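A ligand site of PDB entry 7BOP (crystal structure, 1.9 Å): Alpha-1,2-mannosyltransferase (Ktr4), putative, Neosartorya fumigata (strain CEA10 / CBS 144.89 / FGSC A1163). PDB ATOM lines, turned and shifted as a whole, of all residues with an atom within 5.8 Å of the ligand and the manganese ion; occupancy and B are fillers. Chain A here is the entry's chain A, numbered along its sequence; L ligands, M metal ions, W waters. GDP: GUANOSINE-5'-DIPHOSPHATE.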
ATOM      1  N   SER A  73      28.212 -10.499  23.420  1.00  0.00           N
ATOM      2  CA  SER A  73      27.648 -10.844  22.121  1.00  0.00           C
ATOM      3  C   SER A  73      26.398 -10.033  21.831  1.00  0.00           C
ATOM      4  O   SER A  73      25.464 -10.040  22.632  1.00  0.00           O
ATOM      5  CB  SER A  73      27.349 -12.345  22.047  1.00  0.00           C
ATOM      6  OG  SER A  73      26.928 -12.735  20.744  1.00  0.00           O
ATOM      7  N   LEU A  74      26.426  -9.300  20.723  1.00  0.00           N
ATOM      8  CA  LEU A  74      25.226  -8.696  20.140  1.00  0.00           C
ATOM      9  C   LEU A  74      24.586  -9.773  19.291  1.00  0.00           C
ATOM     10  O   LEU A  74      25.195 -10.273  18.350  1.00  0.00           O
ATOM     11  CB  LEU A  74      25.559  -7.479  19.280  1.00  0.00           C
ATOM     12  CG  LEU A  74      24.347  -6.721  18.714  1.00  0.00           C
ATOM     13  CD1 LEU A  74      23.632  -5.918  19.805  1.00  0.00           C
ATOM     14  CD2 LEU A  74      24.779  -5.814  17.580  1.00  0.00           C
ATOM     15  N   VAL A  75      23.347 -10.155  19.627  1.00  0.00           N
ATOM     16  CA  VAL A  75      22.732 -11.325  19.015  1.00  0.00           C
ATOM     17  C   VAL A  75      21.204 -11.225  19.084  1.00  0.00           C
ATOM     18  O   VAL A  75      20.651 -10.578  19.990  1.00  0.00           O
ATOM     19  CB  VAL A  75      23.286 -12.626  19.658  1.00  0.00           C
ATOM     20  CG1 VAL A  75      23.022 -12.703  21.159  1.00  0.00           C
ATOM     21  CG2 VAL A  75      22.763 -13.868  18.960  1.00  0.00           C
ATOM     22  N   ARG A  76      20.547 -11.851  18.113  1.00  0.00           N
ATOM     23  CA  ARG A  76      19.089 -11.907  18.020  1.00  0.00           C
ATOM     24  C   ARG A  76      18.550 -13.192  18.642  1.00  0.00           C
ATOM     25  O   ARG A  76      19.238 -14.210  18.706  1.00  0.00           O
ATOM     26  CB  ARG A  76      18.643 -11.806  16.549  1.00  0.00           C
ATOM     27  CG  ARG A  76      18.865 -10.437  15.918  1.00  0.00           C
ATOM     28  CD  ARG A  76      18.772 -10.445  14.396  1.00  0.00           C
ATOM     29  NE  ARG A  76      20.043 -10.867  13.791  1.00  0.00           N
ATOM     30  CZ  ARG A  76      20.574 -10.402  12.646  1.00  0.00           C
ATOM     31  NH1 ARG A  76      19.986  -9.448  11.931  1.00  0.00           N
ATOM     32  NH2 ARG A  76      21.756 -10.897  12.235  1.00  0.00           N
ATOM     33  N   GLU A  79      18.756 -16.242  16.343  1.00  0.00           N
ATOM     34  CA  GLU A  79      20.079 -16.870  16.167  1.00  0.00           C
ATOM     35  C   GLU A  79      20.477 -17.783  17.326  1.00  0.00           C
ATOM     36  O   GLU A  79      21.623 -18.222  17.399  1.00  0.00           O
ATOM     37  CB  GLU A  79      21.138 -15.763  15.965  1.00  0.00           C
ATOM     38  CG  GLU A  79      20.886 -14.908  14.740  1.00  0.00           C
ATOM     39  CD  GLU A  79      21.788 -13.691  14.647  1.00  0.00           C
ATOM     40  OE1 GLU A  79      21.920 -12.939  15.635  1.00  0.00           O
ATOM     41  OE2 GLU A  79      22.328 -13.460  13.556  1.00  0.00           O
ATOM     42  N   PHE A 105      23.638  -8.851  24.341  1.00  0.00           N
ATOM     43  CA  PHE A 105      23.020  -7.574  23.977  1.00  0.00           C
ATOM     44  C   PHE A 105      22.072  -7.754  22.817  1.00  0.00           C
ATOM     45  O   PHE A 105      22.337  -8.556  21.911  1.00  0.00           O
ATOM     46  CB  PHE A 105      24.088  -6.554  23.604  1.00  0.00           C
ATOM     47  CG  PHE A 105      24.979  -6.177  24.748  1.00  0.00           C
ATOM     48  CD1 PHE A 105      24.627  -5.129  25.591  1.00  0.00           C
ATOM     49  CD2 PHE A 105      26.168  -6.858  24.981  1.00  0.00           C
ATOM     50  CE1 PHE A 105      25.456  -4.764  26.646  1.00  0.00           C
ATOM     51  CE2 PHE A 105      26.988  -6.498  26.040  1.00  0.00           C
ATOM     52  CZ  PHE A 105      26.643  -5.450  26.871  1.00  0.00           C
ATOM     53  N   ASN A 106      20.992  -6.992  22.826  1.00  0.00           N
ATOM     54  CA  ASN A 106      19.994  -7.055  21.767  1.00  0.00           C
ATOM     55  C   ASN A 106      19.188  -5.756  21.800  1.00  0.00           C
ATOM     56  O   ASN A 106      18.937  -5.192  22.866  1.00  0.00           O
ATOM     57  CB  ASN A 106      19.114  -8.301  21.969  1.00  0.00           C
ATOM     58  CG  ASN A 106      18.159  -8.573  20.806  1.00  0.00           C
ATOM     59  OD1 ASN A 106      18.084  -7.807  19.843  1.00  0.00           O
ATOM     60  ND2 ASN A 106      17.432  -9.676  20.904  1.00  0.00           N
ATOM     61  N   ASP A 107      18.863  -5.211  20.625  1.00  0.00           N
ATOM     62  CA  ASP A 107      18.005  -4.034  20.526  1.00  0.00           C
ATOM     63  C   ASP A 107      16.571  -4.333  21.014  1.00  0.00           C
ATOM     64  O   ASP A 107      15.887  -3.447  21.505  1.00  0.00           O
ATOM     65  CB  ASP A 107      17.980  -3.473  19.093  1.00  0.00           C
ATOM     66  CG  ASP A 107      17.506  -4.486  18.069  1.00  0.00           C
ATOM     67  OD1 ASP A 107      18.097  -5.577  17.978  1.00  0.00           O
ATOM     68  OD2 ASP A 107      16.547  -4.189  17.342  1.00  0.00           O
ATOM     69  N   LYS A 108      16.148  -5.588  20.882  1.00  0.00           N
ATOM     70  CA  LYS A 108      14.879  -6.079  21.402  1.00  0.00           C
ATOM     71  C   LYS A 108      15.087  -6.947  22.652  1.00  0.00           C
ATOM     72  O   LYS A 108      16.208  -7.374  22.921  1.00  0.00           O
ATOM     73  CB  LYS A 108      14.170  -6.880  20.308  1.00  0.00           C
ATOM     74  CG  LYS A 108      13.847  -6.027  19.093  1.00  0.00           C
ATOM     75  CD  LYS A 108      13.493  -6.863  17.890  1.00  0.00           C
ATOM     76  CE  LYS A 108      13.360  -5.979  16.656  1.00  0.00           C
ATOM     77  NZ  LYS A 108      13.210  -6.827  15.434  1.00  0.00           N
ATOM     78  N   TRP A 136      20.892   2.880  19.419  1.00  0.00           N
ATOM     79  CA  TRP A 136      20.481   2.022  18.307  1.00  0.00           C
ATOM     80  C   TRP A 136      19.818   2.781  17.168  1.00  0.00           C
ATOM     81  O   TRP A 136      20.143   2.547  16.004  1.00  0.00           O
ATOM     82  CB  TRP A 136      19.523   0.937  18.786  1.00  0.00           C
ATOM     83  CG  TRP A 136      19.276  -0.141  17.770  1.00  0.00           C
ATOM     84  CD1 TRP A 136      18.124  -0.379  17.079  1.00  0.00           C
ATOM     85  CD2 TRP A 136      20.211  -1.142  17.349  1.00  0.00           C
ATOM     86  NE1 TRP A 136      18.286  -1.452  16.240  1.00  0.00           N
ATOM     87  CE2 TRP A 136      19.557  -1.945  16.387  1.00  0.00           C
ATOM     88  CE3 TRP A 136      21.540  -1.437  17.687  1.00  0.00           C
ATOM     89  CZ2 TRP A 136      20.192  -3.024  15.759  1.00  0.00           C
ATOM     90  CZ3 TRP A 136      22.167  -2.521  17.063  1.00  0.00           C
ATOM     91  CH2 TRP A 136      21.491  -3.285  16.106  1.00  0.00           C
ATOM     92  N   SER A 166      19.220  -2.314   9.781  1.00  0.00           N
ATOM     93  CA  SER A 166      19.746  -2.957  10.975  1.00  0.00           C
ATOM     94  C   SER A 166      21.242  -3.268  10.905  1.00  0.00           C
ATOM     95  O   SER A 166      21.957  -3.169  11.909  1.00  0.00           O
ATOM     96  CB  SER A 166      18.940  -4.223  11.295  1.00  0.00           C
ATOM     97  OG  SER A 166      19.053  -5.185  10.270  1.00  0.00           O
ATOM     98  N   TYR A 167      21.736  -3.608   9.711  1.00  0.00           N
ATOM     99  CA  TYR A 167      23.166  -3.855   9.543  1.00  0.00           C
ATOM    100  C   TYR A 167      23.974  -2.602   9.848  1.00  0.00           C
ATOM    101  O   TYR A 167      25.003  -2.668  10.547  1.00  0.00           O
ATOM    102  CB  TYR A 167      23.508  -4.383   8.141  1.00  0.00           C
ATOM    103  CG  TYR A 167      24.873  -5.013   8.123  1.00  0.00           C
ATOM    104  CD1 TYR A 167      25.055  -6.336   8.512  1.00  0.00           C
ATOM    105  CD2 TYR A 167      25.993  -4.266   7.763  1.00  0.00           C
ATOM    106  CE1 TYR A 167      26.316  -6.905   8.519  1.00  0.00           C
ATOM    107  CE2 TYR A 167      27.267  -4.836   7.769  1.00  0.00           C
ATOM    108  CZ  TYR A 167      27.407  -6.159   8.152  1.00  0.00           C
ATOM    109  OH  TYR A 167      28.652  -6.737   8.166  1.00  0.00           O
ATOM    110  N   MET A 170      23.911  -1.959  13.584  1.00  0.00           N
ATOM    111  CA  MET A 170      24.859  -2.867  14.202  1.00  0.00           C
ATOM    112  C   MET A 170      26.302  -2.369  14.062  1.00  0.00           C
ATOM    113  O   MET A 170      27.051  -2.366  15.036  1.00  0.00           O
ATOM    114  CB  MET A 170      24.702  -4.281  13.627  1.00  0.00           C
ATOM    115  CG  MET A 170      25.711  -5.284  14.142  1.00  0.00           C
ATOM    116  SD  MET A 170      27.285  -5.233  13.256  1.00  0.00           S
ATOM    117  CE  MET A 170      26.768  -5.801  11.638  1.00  0.00           C
ATOM    118  N   ASN A 174      28.641  -1.362  17.286  1.00  0.00           N
ATOM    119  CA  ASN A 174      29.977  -1.913  17.517  1.00  0.00           C
ATOM    120  C   ASN A 174      31.082  -0.862  17.412  1.00  0.00           C
ATOM    121  O   ASN A 174      32.079  -0.952  18.118  1.00  0.00           O
ATOM    122  CB  ASN A 174      30.257  -3.077  16.565  1.00  0.00           C
ATOM    123  CG  ASN A 174      29.525  -4.350  16.973  1.00  0.00           C
ATOM    124  OD1 ASN A 174      29.523  -4.727  18.126  1.00  0.00           O
ATOM    125  ND2 ASN A 174      28.928  -5.008  16.001  1.00  0.00           N
ATOM    126  N   ARG A 192      34.485 -10.283  22.227  1.00  0.00           N
ATOM    127  CA  ARG A 192      33.300 -10.270  21.382  1.00  0.00           C
ATOM    128  C   ARG A 192      33.141 -11.607  20.669  1.00  0.00           C
ATOM    129  O   ARG A 192      34.077 -12.119  20.055  1.00  0.00           O
ATOM    130  CB  ARG A 192      33.385  -9.131  20.367  1.00  0.00           C
ATOM    131  CG  ARG A 192      32.277  -9.173  19.322  1.00  0.00           C
ATOM    132  CD  ARG A 192      32.261  -7.905  18.501  1.00  0.00           C
ATOM    133  NE  ARG A 192      31.572  -8.093  17.231  1.00  0.00           N
ATOM    134  CZ  ARG A 192      31.621  -7.247  16.205  1.00  0.00           C
ATOM    135  NH1 ARG A 192      32.330  -6.119  16.282  1.00  0.00           N
ATOM    136  NH2 ARG A 192      30.958  -7.538  15.086  1.00  0.00           N
ATOM    137  N   VAL A 193      31.926 -12.141  20.730  1.00  0.00           N
ATOM    138  CA  VAL A 193      31.574 -13.418  20.147  1.00  0.00           C
ATOM    139  C   VAL A 193      30.335 -13.229  19.264  1.00  0.00           C
ATOM    140  O   VAL A 193      29.423 -12.491  19.626  1.00  0.00           O
ATOM    141  CB  VAL A 193      31.239 -14.432  21.261  1.00  0.00           C
ATOM    142  CG1 VAL A 193      30.952 -15.807  20.680  1.00  0.00           C
ATOM    143  CG2 VAL A 193      32.374 -14.498  22.272  1.00  0.00           C
ATOM    144  N   GLU A 194      30.328 -13.918  18.117  1.00  0.00           N
ATOM    145  CA  GLU A 194      29.168 -13.965  17.245  1.00  0.00           C
ATOM    146  C   GLU A 194      28.610 -15.373  17.162  1.00  0.00           C
ATOM    147  O   GLU A 194      29.360 -16.332  17.323  1.00  0.00           O
ATOM    148  CB  GLU A 194      29.530 -13.540  15.819  1.00  0.00           C
ATOM    149  CG  GLU A 194      29.791 -12.051  15.673  1.00  0.00           C
ATOM    150  CD  GLU A 194      29.682 -11.518  14.244  1.00  0.00           C
ATOM    151  OE1 GLU A 194      30.057 -10.332  14.143  1.00  0.00           O
ATOM    152  OE2 GLU A 194      29.257 -12.226  13.268  1.00  0.00           O
ATOM    153  N   PRO A 195      27.310 -15.513  16.864  1.00  0.00           N
ATOM    154  CA  PRO A 195      26.763 -16.844  16.594  1.00  0.00           C
ATOM    155  C   PRO A 195      27.339 -17.471  15.324  1.00  0.00           C
ATOM    156  O   PRO A 195      27.804 -16.753  14.448  1.00  0.00           O
ATOM    157  CB  PRO A 195      25.257 -16.584  16.450  1.00  0.00           C
ATOM    158  CG  PRO A 195      25.160 -15.166  16.041  1.00  0.00           C
ATOM    159  CD  PRO A 195      26.296 -14.449  16.699  1.00  0.00           C
ATOM    160  N   ASN A 282      34.310  -9.738  13.958  1.00  0.00           N
ATOM    161  CA  ASN A 282      33.443 -10.771  14.558  1.00  0.00           C
ATOM    162  C   ASN A 282      34.124 -11.473  15.754  1.00  0.00           C
ATOM    163  O   ASN A 282      33.449 -11.894  16.694  1.00  0.00           O
ATOM    164  CB  ASN A 282      32.913 -11.776  13.535  1.00  0.00           C
ATOM    165  CG  ASN A 282      34.001 -12.349  12.657  1.00  0.00           C
ATOM    166  OD1 ASN A 282      34.847 -13.122  13.093  1.00  0.00           O
ATOM    167  ND2 ASN A 282      33.969 -11.969  11.390  1.00  0.00           N
ATOM    168  N   HIS A 343      34.799 -18.044  11.257  1.00  0.00           N
ATOM    169  CA  HIS A 343      33.498 -17.453  10.893  1.00  0.00           C
ATOM    170  C   HIS A 343      33.479 -17.643   9.386  1.00  0.00           C
ATOM    171  O   HIS A 343      34.441 -17.293   8.719  1.00  0.00           O
ATOM    172  CB  HIS A 343      33.439 -15.951  11.281  1.00  0.00           C
ATOM    173  CG  HIS A 343      32.115 -15.258  11.000  1.00  0.00           C
ATOM    174  ND1 HIS A 343      31.656 -15.005   9.723  1.00  0.00           N
ATOM    175  CD2 HIS A 343      31.204 -14.691  11.836  1.00  0.00           C
ATOM    176  CE1 HIS A 343      30.504 -14.353   9.782  1.00  0.00           C
ATOM    177  NE2 HIS A 343      30.209 -14.138  11.058  1.00  0.00           N
HETATM  178  PB  GDP L   1      28.209 -10.555   9.384  1.00  0.00           P
HETATM  179  O1B GDP L   1      27.584 -11.357   8.278  1.00  0.00           O
HETATM  180  O2B GDP L   1      28.971 -11.386  10.424  1.00  0.00           O
HETATM  181  O3B GDP L   1      28.958  -9.306   8.953  1.00  0.00           O
HETATM  182  O3A GDP L   1      26.882  -9.964  10.118  1.00  0.00           O
HETATM  183  PA  GDP L   1      26.004 -10.739  11.256  1.00  0.00           P
HETATM  184  O1A GDP L   1      24.584 -10.910  10.759  1.00  0.00           O
HETATM  185  O2A GDP L   1      26.827 -11.936  11.768  1.00  0.00           O
HETATM  186  O5' GDP L   1      25.971  -9.534  12.316  1.00  0.00           O
HETATM  187  C5' GDP L   1      27.125  -9.216  13.112  1.00  0.00           C
HETATM  188  C4' GDP L   1      26.801  -9.399  14.589  1.00  0.00           C
HETATM  189  O4' GDP L   1      25.772  -8.491  14.961  1.00  0.00           O
HETATM  190  C3' GDP L   1      26.259 -10.780  14.954  1.00  0.00           C
HETATM  191  O3' GDP L   1      26.680 -11.061  16.300  1.00  0.00           O
HETATM  192  C2' GDP L   1      24.751 -10.639  14.833  1.00  0.00           C
HETATM  193  O2' GDP L   1      24.064 -11.544  15.696  1.00  0.00           O
HETATM  194  C1' GDP L   1      24.550  -9.181  15.242  1.00  0.00           C
HETATM  195  N9  GDP L   1      23.451  -8.413  14.608  1.00  0.00           N
HETATM  196  C8  GDP L   1      23.359  -7.953  13.325  1.00  0.00           C
HETATM  197  N7  GDP L   1      22.228  -7.245  13.163  1.00  0.00           N
HETATM  198  C5  GDP L   1      21.570  -7.238  14.350  1.00  0.00           C
HETATM  199  C6  GDP L   1      20.316  -6.677  14.884  1.00  0.00           C
HETATM  200  O6  GDP L   1      19.575  -6.018  14.128  1.00  0.00           O
HETATM  201  N1  GDP L   1      20.002  -6.882  16.175  1.00  0.00           N
HETATM  202  C2  GDP L   1      20.818  -7.594  17.011  1.00  0.00           C
HETATM  203  N2  GDP L   1      20.462  -7.793  18.304  1.00  0.00           N
HETATM  204  N3  GDP L   1      21.984  -8.143  16.575  1.00  0.00           N
HETATM  205  C4  GDP L   1      22.390  -7.993  15.293  1.00  0.00           C
HETATM  206 MN    MN M   1      28.526 -12.900  11.553  1.00  0.00          MN
HETATM  207  O   HOH W   1      31.839 -10.547  10.262  1.00  0.00           O
HETATM  208  O   HOH W   2      27.452 -13.991   9.777  1.00  0.00           O
HETATM  209  O   HOH W   3      28.548  -9.857  18.665  1.00  0.00           O
HETATM  210  O   HOH W   4      24.767 -13.806  12.522  1.00  0.00           O
HETATM  211  O   HOH W   5      27.427 -14.640  12.736  1.00  0.00           O
HETATM  212  O   HOH W   6      17.161  -4.996  14.692  1.00  0.00           O
HETATM  213  O   HOH W   7      22.661  -9.136   9.748  1.00  0.00           O
HETATM  214  O   HOH W   8      21.534  -6.534  10.598  1.00  0.00           O
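OE1 of Glu 79 lies within hydrogen-bond range of O2' of the ligand (2.6 Å). N2 of the ligand lies within hydrogen-bond range of O of Val 75, 3.3 Å away. O1A of the ligand is in salt-bridge range of NH2 of Arg 76 (3.2 Å). N2 of the ligand is in hydrogen-bond range of OD1 of Asn 106. A nitrogen (N1) of the ligand is in hydrogen-bond range of the side-chain carboxylate (OD1) of Asp 107, 2.9 Å away. OH of Tyr 167 lies within hydrogen-bond range of O3B of the ligand, 2.7 Å away. An oxygen (O3') of the ligand is in hydrogen-bond range of the backbone carbonyl oxygen of Leu 74.
The backbone carbonyl oxygen (O) of Phe 105 sits at hydrogen-bond distance from the backbone NH (N) of Val 75. The side-chain sulfur (SD) of Met 170 sits at hydrogen-bond distance from the side-chain amide nitrogen (ND2) of Asn 174 (3.2 Å). OE1 of Glu 194 is in salt-bridge range of NH2 of Arg 192 (3.1 Å). ND2 of Asn 106 lies close to O of Val 75 (3.5 Å). The side-chain amide oxygen (OD1) of Asn 106 lies close to the side-chain carboxylate (OD1) of Asp 107 (2.9 Å). The side-chain carboxylate (OE2) of Glu 79 lies within salt-bridge range of the guanidinium group (NH2) of Arg 76 (2.9 Å). The side-chain carboxylate (OD2) of Asp 107 is in hydrogen-bond range of the indole nitrogen (NE1) of Trp 136 (3.4 Å). OD1 of Asn 106 is in hydrogen-bond range of N of Lys 108 (3.1 Å).
Trp 136 touches the ligand. Ser 166 touches the ligand. Met 170 touches the ligand (CG to O4', 3.3 Å). Pro 195 touches the ligand. Hydrophobic or aromatic side chains within 4 Å of the ligand: Leu 74, Trp 136, Tyr 167, Met 170, Pro 195 and His 343. Within 4 Å of the ligand: Leu 74, Val 75, Arg 76, Glu 79, Asn 106, Asp 107, Trp 136, Ser 166, Tyr 167, Met 170, Glu 194, Pro 195 and His 343.
Of the 20 residues printed, 2 come within 4 Å of the manganese ion.
The manganese ion is bound by O2B of the ligand, O2A of the ligand, OE2 of Glu 194, NE2 of His 343, water W2 and water W5.
Water W6 bridges O6 of the ligand (2.7 Å) and OD2 of Asp 107 (2.8 Å). Water W8 lies within hydrogen-bond range of a nitrogen (N7) of the ligand (2.8 Å), the side-chain hydroxyl of Ser 166 (2.8 Å) and the backbone NH of Tyr 167 (3.1 Å). Water W7 bridges O1A of the ligand and NH2 of Arg 76. Water W4 lies within hydrogen-bond range of OE2 of Glu 79 (2.7 Å) and O1A of the ligand (3.4 Å). Water W1 lies within hydrogen-bond range of ND2 of Asn 282 (2.8 Å) and O3B of the ligand (3.4 Å). Water W3 lies within hydrogen-bond range of O of Val 193, N of Leu 74 and O3' of the ligand.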
